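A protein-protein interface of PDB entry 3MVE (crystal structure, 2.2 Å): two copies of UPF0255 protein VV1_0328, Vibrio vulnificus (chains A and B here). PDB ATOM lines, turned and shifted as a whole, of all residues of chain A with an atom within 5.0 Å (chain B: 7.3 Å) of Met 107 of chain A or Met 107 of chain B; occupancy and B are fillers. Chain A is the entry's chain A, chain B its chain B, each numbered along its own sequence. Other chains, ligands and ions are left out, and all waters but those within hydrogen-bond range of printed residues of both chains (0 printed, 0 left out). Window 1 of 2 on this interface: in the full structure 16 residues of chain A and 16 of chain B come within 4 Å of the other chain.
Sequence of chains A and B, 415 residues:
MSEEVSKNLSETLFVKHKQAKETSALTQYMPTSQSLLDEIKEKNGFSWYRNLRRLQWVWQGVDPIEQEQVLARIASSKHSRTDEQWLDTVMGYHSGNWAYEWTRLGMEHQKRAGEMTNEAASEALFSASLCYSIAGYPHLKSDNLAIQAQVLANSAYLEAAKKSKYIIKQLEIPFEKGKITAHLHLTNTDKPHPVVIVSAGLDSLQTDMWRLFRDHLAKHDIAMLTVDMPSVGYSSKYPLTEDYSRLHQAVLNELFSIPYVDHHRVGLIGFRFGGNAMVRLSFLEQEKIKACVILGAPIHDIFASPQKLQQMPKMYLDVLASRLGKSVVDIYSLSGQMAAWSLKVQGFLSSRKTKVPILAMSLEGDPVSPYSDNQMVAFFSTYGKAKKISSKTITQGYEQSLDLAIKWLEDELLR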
ATOM      1  N   THR A 103      -8.160  10.668 -40.449  1.00  0.00           N
ATOM      2  CA  THR A 103      -8.358  10.400 -39.027  1.00  0.00           C
ATOM      3  C   THR A 103      -7.788  11.565 -38.220  1.00  0.00           C
ATOM      4  O   THR A 103      -8.350  11.931 -37.187  1.00  0.00           O
ATOM      5  CB  THR A 103      -7.689   9.074 -38.586  1.00  0.00           C
ATOM      6  OG1 THR A 103      -8.306   7.983 -39.288  1.00  0.00           O
ATOM      7  CG2 THR A 103      -7.864   8.851 -37.087  1.00  0.00           C
ATOM      8  N   ARG A 104      -6.688  12.162 -38.692  1.00  0.00           N
ATOM      9  CA  ARG A 104      -6.109  13.304 -37.990  1.00  0.00           C
ATOM     10  C   ARG A 104      -7.135  14.442 -37.906  1.00  0.00           C
ATOM     11  O   ARG A 104      -7.308  15.054 -36.853  1.00  0.00           O
ATOM     12  CB  ARG A 104      -4.840  13.793 -38.695  1.00  0.00           C
ATOM     13  N   LEU A 105      -7.820  14.723 -39.010  1.00  0.00           N
ATOM     14  CA  LEU A 105      -8.828  15.781 -39.026  1.00  0.00           C
ATOM     15  C   LEU A 105      -9.991  15.408 -38.110  1.00  0.00           C
ATOM     16  O   LEU A 105     -10.513  16.238 -37.357  1.00  0.00           O
ATOM     17  CB  LEU A 105      -9.335  16.007 -40.461  1.00  0.00           C
ATOM     18  CG  LEU A 105     -10.378  17.099 -40.678  1.00  0.00           C
ATOM     19  CD1 LEU A 105      -9.875  18.431 -40.094  1.00  0.00           C
ATOM     20  CD2 LEU A 105     -10.682  17.226 -42.168  1.00  0.00           C
ATOM     21  N   GLY A 106     -10.404  14.151 -38.162  1.00  0.00           N
ATOM     22  CA  GLY A 106     -11.496  13.727 -37.302  1.00  0.00           C
ATOM     23  C   GLY A 106     -11.136  13.959 -35.842  1.00  0.00           C
ATOM     24  O   GLY A 106     -11.964  14.418 -35.043  1.00  0.00           O
ATOM     25  N   MET A 107      -9.891  13.651 -35.480  1.00  0.00           N
ATOM     26  CA  MET A 107      -9.449  13.844 -34.103  1.00  0.00           C
ATOM     27  C   MET A 107      -9.489  15.318 -33.698  1.00  0.00           C
ATOM     28  O   MET A 107      -9.898  15.634 -32.574  1.00  0.00           O
ATOM     29  CB  MET A 107      -8.050  13.250 -33.895  1.00  0.00           C
ATOM     30  CG  MET A 107      -8.055  11.718 -33.836  1.00  0.00           C
ATOM     31  SD  MET A 107      -6.412  10.953 -33.625  1.00  0.00           S
ATOM     32  CE  MET A 107      -6.027  11.453 -31.962  1.00  0.00           C
ATOM     33  N   GLU A 108      -9.100  16.218 -34.607  1.00  0.00           N
ATOM     34  CA  GLU A 108      -9.127  17.649 -34.302  1.00  0.00           C
ATOM     35  C   GLU A 108     -10.542  18.089 -33.964  1.00  0.00           C
ATOM     36  O   GLU A 108     -10.766  18.766 -32.964  1.00  0.00           O
ATOM     37  CB  GLU A 108      -8.608  18.497 -35.475  1.00  0.00           C
ATOM     38  CG  GLU A 108      -7.168  18.235 -35.898  1.00  0.00           C
ATOM     39  CD  GLU A 108      -6.574  19.381 -36.746  1.00  0.00           C
ATOM     40  OE1 GLU A 108      -5.663  19.123 -37.573  1.00  0.00           O
ATOM     41  OE2 GLU A 108      -7.009  20.543 -36.575  1.00  0.00           O
ATOM     42  N   HIS A 109     -11.497  17.706 -34.809  1.00  0.00           N
ATOM     43  CA  HIS A 109     -12.900  18.042 -34.595  1.00  0.00           C
ATOM     44  C   HIS A 109     -13.370  17.457 -33.268  1.00  0.00           C
ATOM     45  O   HIS A 109     -14.103  18.107 -32.504  1.00  0.00           O
ATOM     46  CB  HIS A 109     -13.766  17.486 -35.743  1.00  0.00           C
ATOM     47  CG  HIS A 109     -13.762  18.346 -36.970  1.00  0.00           C
ATOM     48  ND1 HIS A 109     -14.264  19.632 -36.975  1.00  0.00           N
ATOM     49  CD2 HIS A 109     -13.279  18.126 -38.217  1.00  0.00           C
ATOM     50  CE1 HIS A 109     -14.081  20.166 -38.171  1.00  0.00           C
ATOM     51  NE2 HIS A 109     -13.486  19.274 -38.943  1.00  0.00           N
ATOM     52  N   GLN A 110     -12.953  16.227 -32.991  1.00  0.00           N
ATOM     53  CA  GLN A 110     -13.357  15.603 -31.748  1.00  0.00           C
ATOM     54  C   GLN A 110     -12.822  16.406 -30.567  1.00  0.00           C
ATOM     55  O   GLN A 110     -13.531  16.617 -29.592  1.00  0.00           O
ATOM     56  CB  GLN A 110     -12.866  14.157 -31.656  1.00  0.00           C
ATOM     57  CG  GLN A 110     -13.442  13.441 -30.425  1.00  0.00           C
ATOM     58  CD  GLN A 110     -13.313  11.944 -30.496  1.00  0.00           C
ATOM     59  OE1 GLN A 110     -13.497  11.341 -31.560  1.00  0.00           O
ATOM     60  NE2 GLN A 110     -13.008  11.326 -29.360  1.00  0.00           N
ATOM     61  N   LYS A 111     -11.580  16.873 -30.671  1.00  0.00           N
ATOM     62  CA  LYS A 111     -10.970  17.663 -29.600  1.00  0.00           C
ATOM     63  C   LYS A 111     -11.688  18.993 -29.379  1.00  0.00           C
ATOM     64  O   LYS A 111     -11.931  19.392 -28.235  1.00  0.00           O
ATOM     65  CB  LYS A 111      -9.483  17.908 -29.897  1.00  0.00           C
ATOM     66  CG  LYS A 111      -8.887  19.087 -29.125  1.00  0.00           C
ATOM     67  CD  LYS A 111      -7.382  18.992 -28.967  1.00  0.00           C
ATOM     68  CE  LYS A 111      -6.654  18.840 -30.303  1.00  0.00           C
ATOM     69  NZ  LYS A 111      -6.695  20.070 -31.164  1.00  0.00           N
ATOM     70  N   TYR A 132     -13.888  10.268 -39.795  1.00  0.00           N
ATOM     71  CA  TYR A 132     -13.405   8.907 -39.533  1.00  0.00           C
ATOM     72  C   TYR A 132     -13.939   7.943 -40.602  1.00  0.00           C
ATOM     73  O   TYR A 132     -13.249   6.991 -41.018  1.00  0.00           O
ATOM     74  CB  TYR A 132     -13.856   8.426 -38.149  1.00  0.00           C
ATOM     75  CG  TYR A 132     -13.279   9.221 -36.990  1.00  0.00           C
ATOM     76  CD1 TYR A 132     -11.941   9.637 -36.998  1.00  0.00           C
ATOM     77  CD2 TYR A 132     -14.057   9.522 -35.863  1.00  0.00           C
ATOM     78  CE1 TYR A 132     -11.381  10.333 -35.911  1.00  0.00           C
ATOM     79  CE2 TYR A 132     -13.512  10.221 -34.767  1.00  0.00           C
ATOM     80  CZ  TYR A 132     -12.174  10.626 -34.799  1.00  0.00           C
ATOM     81  OH  TYR A 132     -11.635  11.337 -33.739  1.00  0.00           O
ATOM     82  N   TYR B  93     -19.122  14.642 -22.427  1.00  0.00           N
ATOM     83  CA  TYR B  93     -17.821  14.486 -23.062  1.00  0.00           C
ATOM     84  C   TYR B  93     -17.354  15.893 -23.397  1.00  0.00           C
ATOM     85  O   TYR B  93     -17.664  16.429 -24.457  1.00  0.00           O
ATOM     86  CB  TYR B  93     -17.901  13.657 -24.349  1.00  0.00           C
ATOM     87  CG  TYR B  93     -16.535  13.443 -24.991  1.00  0.00           C
ATOM     88  CD1 TYR B  93     -15.552  12.673 -24.355  1.00  0.00           C
ATOM     89  CD2 TYR B  93     -16.230  13.991 -26.240  1.00  0.00           C
ATOM     90  CE1 TYR B  93     -14.316  12.450 -24.948  1.00  0.00           C
ATOM     91  CE2 TYR B  93     -14.993  13.776 -26.844  1.00  0.00           C
ATOM     92  CZ  TYR B  93     -14.047  13.003 -26.193  1.00  0.00           C
ATOM     93  OH  TYR B  93     -12.841  12.769 -26.798  1.00  0.00           O
ATOM     94  N   TYR B 100     -11.984  12.419 -21.898  1.00  0.00           N
ATOM     95  CA  TYR B 100     -11.606  13.596 -22.679  1.00  0.00           C
ATOM     96  C   TYR B 100     -10.250  14.203 -22.319  1.00  0.00           C
ATOM     97  O   TYR B 100      -9.442  14.474 -23.197  1.00  0.00           O
ATOM     98  CB  TYR B 100     -12.670  14.693 -22.565  1.00  0.00           C
ATOM     99  CG  TYR B 100     -12.353  15.929 -23.393  1.00  0.00           C
ATOM    100  CD1 TYR B 100     -12.424  15.892 -24.788  1.00  0.00           C
ATOM    101  CD2 TYR B 100     -11.978  17.134 -22.782  1.00  0.00           C
ATOM    102  CE1 TYR B 100     -12.138  17.020 -25.552  1.00  0.00           C
ATOM    103  CE2 TYR B 100     -11.682  18.273 -23.540  1.00  0.00           C
ATOM    104  CZ  TYR B 100     -11.770  18.199 -24.932  1.00  0.00           C
ATOM    105  OH  TYR B 100     -11.495  19.303 -25.704  1.00  0.00           O
ATOM    106  N   GLU B 101     -10.007  14.428 -21.029  1.00  0.00           N
ATOM    107  CA  GLU B 101      -8.761  15.048 -20.593  1.00  0.00           C
ATOM    108  C   GLU B 101      -7.554  14.169 -20.909  1.00  0.00           C
ATOM    109  O   GLU B 101      -6.519  14.658 -21.356  1.00  0.00           O
ATOM    110  CB  GLU B 101      -8.828  15.370 -19.098  1.00  0.00           C
ATOM    111  CG  GLU B 101      -9.921  16.375 -18.690  1.00  0.00           C
ATOM    112  CD  GLU B 101      -9.701  17.787 -19.238  1.00  0.00           C
ATOM    113  OE1 GLU B 101      -8.611  18.074 -19.771  1.00  0.00           O
ATOM    114  OE2 GLU B 101     -10.624  18.626 -19.133  1.00  0.00           O
ATOM    115  N   TRP B 102      -7.688  12.867 -20.696  1.00  0.00           N
ATOM    116  CA  TRP B 102      -6.600  11.950 -20.995  1.00  0.00           C
ATOM    117  C   TRP B 102      -6.385  11.844 -22.496  1.00  0.00           C
ATOM    118  O   TRP B 102      -5.262  11.687 -22.968  1.00  0.00           O
ATOM    119  CB  TRP B 102      -6.877  10.564 -20.409  1.00  0.00           C
ATOM    120  CG  TRP B 102      -6.499  10.444 -18.971  1.00  0.00           C
ATOM    121  CD1 TRP B 102      -7.342  10.460 -17.898  1.00  0.00           C
ATOM    122  CD2 TRP B 102      -5.168  10.320 -18.440  1.00  0.00           C
ATOM    123  NE1 TRP B 102      -6.618  10.355 -16.728  1.00  0.00           N
ATOM    124  CE2 TRP B 102      -5.283  10.270 -17.034  1.00  0.00           C
ATOM    125  CE3 TRP B 102      -3.893  10.247 -19.021  1.00  0.00           C
ATOM    126  CZ2 TRP B 102      -4.168  10.151 -16.193  1.00  0.00           C
ATOM    127  CZ3 TRP B 102      -2.779  10.130 -18.186  1.00  0.00           C
ATOM    128  CH2 TRP B 102      -2.928  10.084 -16.783  1.00  0.00           C
ATOM    129  N   THR B 103      -7.470  11.914 -23.255  1.00  0.00           N
ATOM    130  CA  THR B 103      -7.371  11.856 -24.711  1.00  0.00           C
ATOM    131  C   THR B 103      -6.668  13.117 -25.205  1.00  0.00           C
ATOM    132  O   THR B 103      -5.833  13.059 -26.127  1.00  0.00           O
ATOM    133  CB  THR B 103      -8.771  11.696 -25.353  1.00  0.00           C
ATOM    134  OG1 THR B 103      -9.320  10.440 -24.946  1.00  0.00           O
ATOM    135  CG2 THR B 103      -8.681  11.669 -26.871  1.00  0.00           C
ATOM    136  N   ARG B 104      -6.963  14.257 -24.583  1.00  0.00           N
ATOM    137  CA  ARG B 104      -6.291  15.497 -24.983  1.00  0.00           C
ATOM    138  C   ARG B 104      -4.781  15.406 -24.777  1.00  0.00           C
ATOM    139  O   ARG B 104      -4.000  15.921 -25.583  1.00  0.00           O
ATOM    140  CB  ARG B 104      -6.865  16.697 -24.202  1.00  0.00           C
ATOM    141  N   LEU B 105      -4.355  14.744 -23.705  1.00  0.00           N
ATOM    142  CA  LEU B 105      -2.915  14.616 -23.469  1.00  0.00           C
ATOM    143  C   LEU B 105      -2.329  13.696 -24.538  1.00  0.00           C
ATOM    144  O   LEU B 105      -1.293  13.985 -25.107  1.00  0.00           O
ATOM    145  CB  LEU B 105      -2.641  14.043 -22.075  1.00  0.00           C
ATOM    146  CG  LEU B 105      -1.168  13.729 -21.757  1.00  0.00           C
ATOM    147  CD1 LEU B 105      -0.304  14.983 -21.933  1.00  0.00           C
ATOM    148  CD2 LEU B 105      -1.086  13.261 -20.317  1.00  0.00           C
ATOM    149  N   GLY B 106      -3.016  12.601 -24.816  1.00  0.00           N
ATOM    150  CA  GLY B 106      -2.513  11.694 -25.825  1.00  0.00           C
ATOM    151  C   GLY B 106      -2.365  12.399 -27.160  1.00  0.00           C
ATOM    152  O   GLY B 106      -1.374  12.207 -27.874  1.00  0.00           O
ATOM    153  N   MET B 107      -3.348  13.229 -27.505  1.00  0.00           N
ATOM    154  CA  MET B 107      -3.282  13.961 -28.761  1.00  0.00           C
ATOM    155  C   MET B 107      -2.098  14.911 -28.768  1.00  0.00           C
ATOM    156  O   MET B 107      -1.451  15.075 -29.787  1.00  0.00           O
ATOM    157  CB  MET B 107      -4.573  14.747 -29.022  1.00  0.00           C
ATOM    158  CG  MET B 107      -5.777  13.865 -29.336  1.00  0.00           C
ATOM    159  SD  MET B 107      -7.226  14.825 -29.825  1.00  0.00           S
ATOM    160  CE  MET B 107      -8.382  13.522 -30.358  1.00  0.00           C
ATOM    161  N   GLU B 108      -1.809  15.532 -27.630  1.00  0.00           N
ATOM    162  CA  GLU B 108      -0.692  16.462 -27.557  1.00  0.00           C
ATOM    163  C   GLU B 108       0.623  15.740 -27.876  1.00  0.00           C
ATOM    164  O   GLU B 108       1.466  16.271 -28.601  1.00  0.00           O
ATOM    165  CB  GLU B 108      -0.633  17.110 -26.172  1.00  0.00           C
ATOM    166  CG  GLU B 108       0.003  18.485 -26.166  1.00  0.00           C
ATOM    167  CD  GLU B 108      -0.739  19.486 -27.052  1.00  0.00           C
ATOM    168  OE1 GLU B 108      -1.964  19.668 -26.858  1.00  0.00           O
ATOM    169  OE2 GLU B 108      -0.098  20.095 -27.941  1.00  0.00           O
ATOM    170  N   HIS B 109       0.793  14.533 -27.341  1.00  0.00           N
ATOM    171  CA  HIS B 109       1.997  13.743 -27.609  1.00  0.00           C
ATOM    172  C   HIS B 109       2.064  13.361 -29.086  1.00  0.00           C
ATOM    173  O   HIS B 109       3.111  13.464 -29.724  1.00  0.00           O
ATOM    174  CB  HIS B 109       1.985  12.449 -26.789  1.00  0.00           C
ATOM    175  CG  HIS B 109       2.493  12.603 -25.391  1.00  0.00           C
ATOM    176  ND1 HIS B 109       3.828  12.804 -25.103  1.00  0.00           N
ATOM    177  CD2 HIS B 109       1.851  12.572 -24.199  1.00  0.00           C
ATOM    178  CE1 HIS B 109       3.985  12.887 -23.794  1.00  0.00           C
ATOM    179  NE2 HIS B 109       2.802  12.751 -23.221  1.00  0.00           N
ATOM    180  N   GLN B 110       0.931  12.898 -29.608  1.00  0.00           N
ATOM    181  CA  GLN B 110       0.802  12.456 -30.993  1.00  0.00           C
ATOM    182  C   GLN B 110       1.023  13.575 -32.010  1.00  0.00           C
ATOM    183  O   GLN B 110       1.646  13.351 -33.050  1.00  0.00           O
ATOM    184  CB  GLN B 110      -0.580  11.810 -31.183  1.00  0.00           C
ATOM    185  CG  GLN B 110      -0.895  11.274 -32.569  1.00  0.00           C
ATOM    186  CD  GLN B 110      -2.007  10.225 -32.548  1.00  0.00           C
ATOM    187  OE1 GLN B 110      -2.962  10.334 -31.781  1.00  0.00           O
ATOM    188  NE2 GLN B 110      -1.888   9.210 -33.398  1.00  0.00           N
ATOM    189  N   LYS B 111       0.528  14.775 -31.709  1.00  0.00           N
ATOM    190  CA  LYS B 111       0.678  15.914 -32.614  1.00  0.00           C
ATOM    191  C   LYS B 111       2.145  16.301 -32.733  1.00  0.00           C
ATOM    192  O   LYS B 111       2.683  16.448 -33.831  1.00  0.00           O
ATOM    193  CB  LYS B 111      -0.130  17.106 -32.101  1.00  0.00           C
ATOM    194  N   ARG B 112       2.780  16.463 -31.578  1.00  0.00           N
ATOM    195  CA  ARG B 112       4.184  16.831 -31.495  1.00  0.00           C
ATOM    196  C   ARG B 112       5.085  15.912 -32.323  1.00  0.00           C
ATOM    197  O   ARG B 112       6.106  16.353 -32.851  1.00  0.00           O
ATOM    198  CB  ARG B 112       4.628  16.827 -30.024  1.00  0.00           C
ATOM    199  N   ALA B 113       4.710  14.639 -32.431  1.00  0.00           N
ATOM    200  CA  ALA B 113       5.481  13.660 -33.194  1.00  0.00           C
ATOM    201  C   ALA B 113       5.538  14.018 -34.681  1.00  0.00           C
ATOM    202  O   ALA B 113       6.208  13.344 -35.472  1.00  0.00           O
ATOM    203  CB  ALA B 113       4.873  12.271 -33.012  1.00  0.00           C
ATOM    204  N   ALA B 128       1.563   8.431 -26.477  1.00  0.00           N
ATOM    205  CA  ALA B 128       0.209   8.738 -26.907  1.00  0.00           C
ATOM    206  C   ALA B 128      -0.696   7.524 -26.643  1.00  0.00           C
ATOM    207  O   ALA B 128      -1.769   7.657 -26.073  1.00  0.00           O
ATOM    208  CB  ALA B 128       0.214   9.079 -28.367  1.00  0.00           C
ATOM    209  N   CYS B 131      -1.715   6.991 -23.027  1.00  0.00           N
ATOM    210  CA  CYS B 131      -2.661   8.005 -22.595  1.00  0.00           C
ATOM    211  C   CYS B 131      -4.060   7.647 -23.045  1.00  0.00           C
ATOM    212  O   CYS B 131      -5.019   7.814 -22.289  1.00  0.00           O
ATOM    213  CB  CYS B 131      -2.252   9.373 -23.142  1.00  0.00           C
ATOM    214  SG  CYS B 131      -0.766  10.056 -22.326  1.00  0.00           S
ATOM    215  N   TYR B 132      -4.173   7.146 -24.273  1.00  0.00           N
ATOM    216  CA  TYR B 132      -5.468   6.735 -24.808  1.00  0.00           C
ATOM    217  C   TYR B 132      -6.001   5.532 -24.014  1.00  0.00           C
ATOM    218  O   TYR B 132      -7.198   5.459 -23.716  1.00  0.00           O
ATOM    219  CB  TYR B 132      -5.345   6.383 -26.300  1.00  0.00           C
ATOM    220  CG  TYR B 132      -4.996   7.567 -27.176  1.00  0.00           C
ATOM    221  CD1 TYR B 132      -5.572   8.818 -26.945  1.00  0.00           C
ATOM    222  CD2 TYR B 132      -4.111   7.440 -28.255  1.00  0.00           C
ATOM    223  CE1 TYR B 132      -5.282   9.913 -27.754  1.00  0.00           C
ATOM    224  CE2 TYR B 132      -3.818   8.541 -29.078  1.00  0.00           C
ATOM    225  CZ  TYR B 132      -4.409   9.769 -28.812  1.00  0.00           C
ATOM    226  OH  TYR B 132      -4.133  10.864 -29.576  1.00  0.00           O
ATOM    227  N   GLN B 148     -13.828   3.524 -28.082  1.00  0.00           N
ATOM    228  CA  GLN B 148     -13.164   4.355 -29.071  1.00  0.00           C
ATOM    229  C   GLN B 148     -11.708   4.615 -28.674  1.00  0.00           C
ATOM    230  O   GLN B 148     -10.810   4.611 -29.518  1.00  0.00           O
ATOM    231  CB  GLN B 148     -13.889   5.700 -29.244  1.00  0.00           C
ATOM    232  CG  GLN B 148     -13.393   6.467 -30.472  1.00  0.00           C
ATOM    233  CD  GLN B 148     -13.742   7.930 -30.435  1.00  0.00           C
ATOM    234  OE1 GLN B 148     -13.549   8.586 -29.413  1.00  0.00           O
ATOM    235  NE2 GLN B 148     -14.247   8.465 -31.561  1.00  0.00           N
ATOM    236  N   LEU B 152      -7.934   4.161 -30.538  1.00  0.00           N
ATOM    237  CA  LEU B 152      -6.894   5.180 -30.555  1.00  0.00           C
ATOM    238  C   LEU B 152      -5.594   4.651 -29.946  1.00  0.00           C
ATOM    239  O   LEU B 152      -4.511   4.955 -30.443  1.00  0.00           O
ATOM    240  CB  LEU B 152      -7.367   6.423 -29.805  1.00  0.00           C
ATOM    241  CG  LEU B 152      -8.614   7.066 -30.431  1.00  0.00           C
ATOM    242  CD1 LEU B 152      -8.996   8.339 -29.687  1.00  0.00           C
ATOM    243  CD2 LEU B 152      -8.315   7.390 -31.874  1.00  0.00           C
ATOM    244  N   SER B 155      -4.034   2.336 -32.737  1.00  0.00           N
ATOM    245  CA  SER B 155      -3.478   3.041 -33.905  1.00  0.00           C
ATOM    246  C   SER B 155      -2.176   3.768 -33.542  1.00  0.00           C
ATOM    247  O   SER B 155      -1.225   3.817 -34.322  1.00  0.00           O
ATOM    248  CB  SER B 155      -4.481   4.072 -34.453  1.00  0.00           C
ATOM    249  OG  SER B 155      -5.643   3.448 -34.937  1.00  0.00           O
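Met 107 of chain A touches its own counterpart, Met 107 of chain B.
Met 107 of chain A touches Gln 110 of chain B, but with the chains exchanged Gln 110 of chain A does not touch Met 107 of chain B (4.7 Å).
Met 107 of chain A touches Tyr 132 of chain B, but with the chains exchanged Tyr 132 of chain A does not touch Met 107 of chain B (5.2 Å).
Lys 111 of chain A touches Met 107 of chain B, but with the chains exchanged Met 107 of chain A does not touch Lys 111 of chain B (7.4 Å).
Of the 8 pairs that touch across the chains among the printed residues, 1 has its exchanged pair printed and touching as well.
The backbone NH (N) of Met 107 of chain A lies close to the side-chain hydroxyl (OH) of Tyr 132 of chain A (3.4 Å).
The side-chain amide oxygen (OE1) of Gln 110 of chain A sits at hydrogen-bond distance from the side-chain hydroxyl (OH) of Tyr 132 of chain A (2.9 Å).
The backbone carbonyl oxygen of Gly 106 of chain A is in hydrogen-bond range of the side-chain hydroxyl of Tyr 132 of chain A (3.4 Å).
OE1 of Gln 110 of chain B sits at hydrogen-bond distance from OH of Tyr 132 of chain B, at 2.6 Å.
The side-chain hydroxyl (OH) of Tyr 132 of chain B is in hydrogen-bond range of the backbone NH (N) of Met 107 of chain B (3.2 Å).
NE2 of Gln 110 of chain A lies within hydrogen-bond range of OH of Tyr 93 of chain B, at 2.9 Å.
The side-chain amide nitrogen (NE2) of Gln 110 of chain A sits at hydrogen-bond distance from the side-chain amide oxygen (OE1) of Gln 148 of chain B (2.8 Å).
The backbone carbonyl oxygen (O) of Lys 111 of chain A sits at hydrogen-bond distance from the side-chain hydroxyl (OH) of Tyr 100 of chain B, at 2.6 Å.
Among the printed residues, merely in contact across the chains: Met 107 of chain A with Met 107 of chain B, Met 107 of chain A with Gln 110 of chain B, Met 107 of chain A with Tyr 132 of chain B, Lys 111 of chain A with Met 107 of chain B and Tyr 132 of chain A with Gln 148 of chain B.
Of the 21 printed residues of chain B, 6 touch a printed residue of chain A.
Among the printed residues, 8 pairs touch across the chains.
Among the printed residues, no Asp or Glu carboxylate lies within 4 Å of a Lys or Arg side-chain nitrogen of the other chain.
No residue of chain B comes within 4 Å of Gly 106 of chain A.
Of chain B, only Met 107, Gln 110 and Tyr 132 come within 4 Å of Met 107 of chain A.
Printed residues of chain B within 4 Å of Gln 110 of chain A: Tyr 93 and Gln 148.
Of the printed residues of chain B, Tyr 132 of chain A touches Gln 148 (3.7 Å).
Thr 103 of chain B touches none of the printed residues of chain A.
Gly 106 of chain B touches none of the printed residues of chain A.
Of chain A, only Met 107 (3.4 Å) and Lys 111 (3.8 Å) come within 4 Å of Met 107 of chain B.
Of the printed residues of chain A, Gln 110 of chain B touches Met 107 (3.3 Å).
Of the printed residues of chain A, Gln 148 of chain B touches Gln 110 (2.8 Å) and Tyr 132 (3.7 Å).
The nearest printed residue of chain A that does not touch Tyr 132 of chain B is Gln 110 of chain A (8.0 Å).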
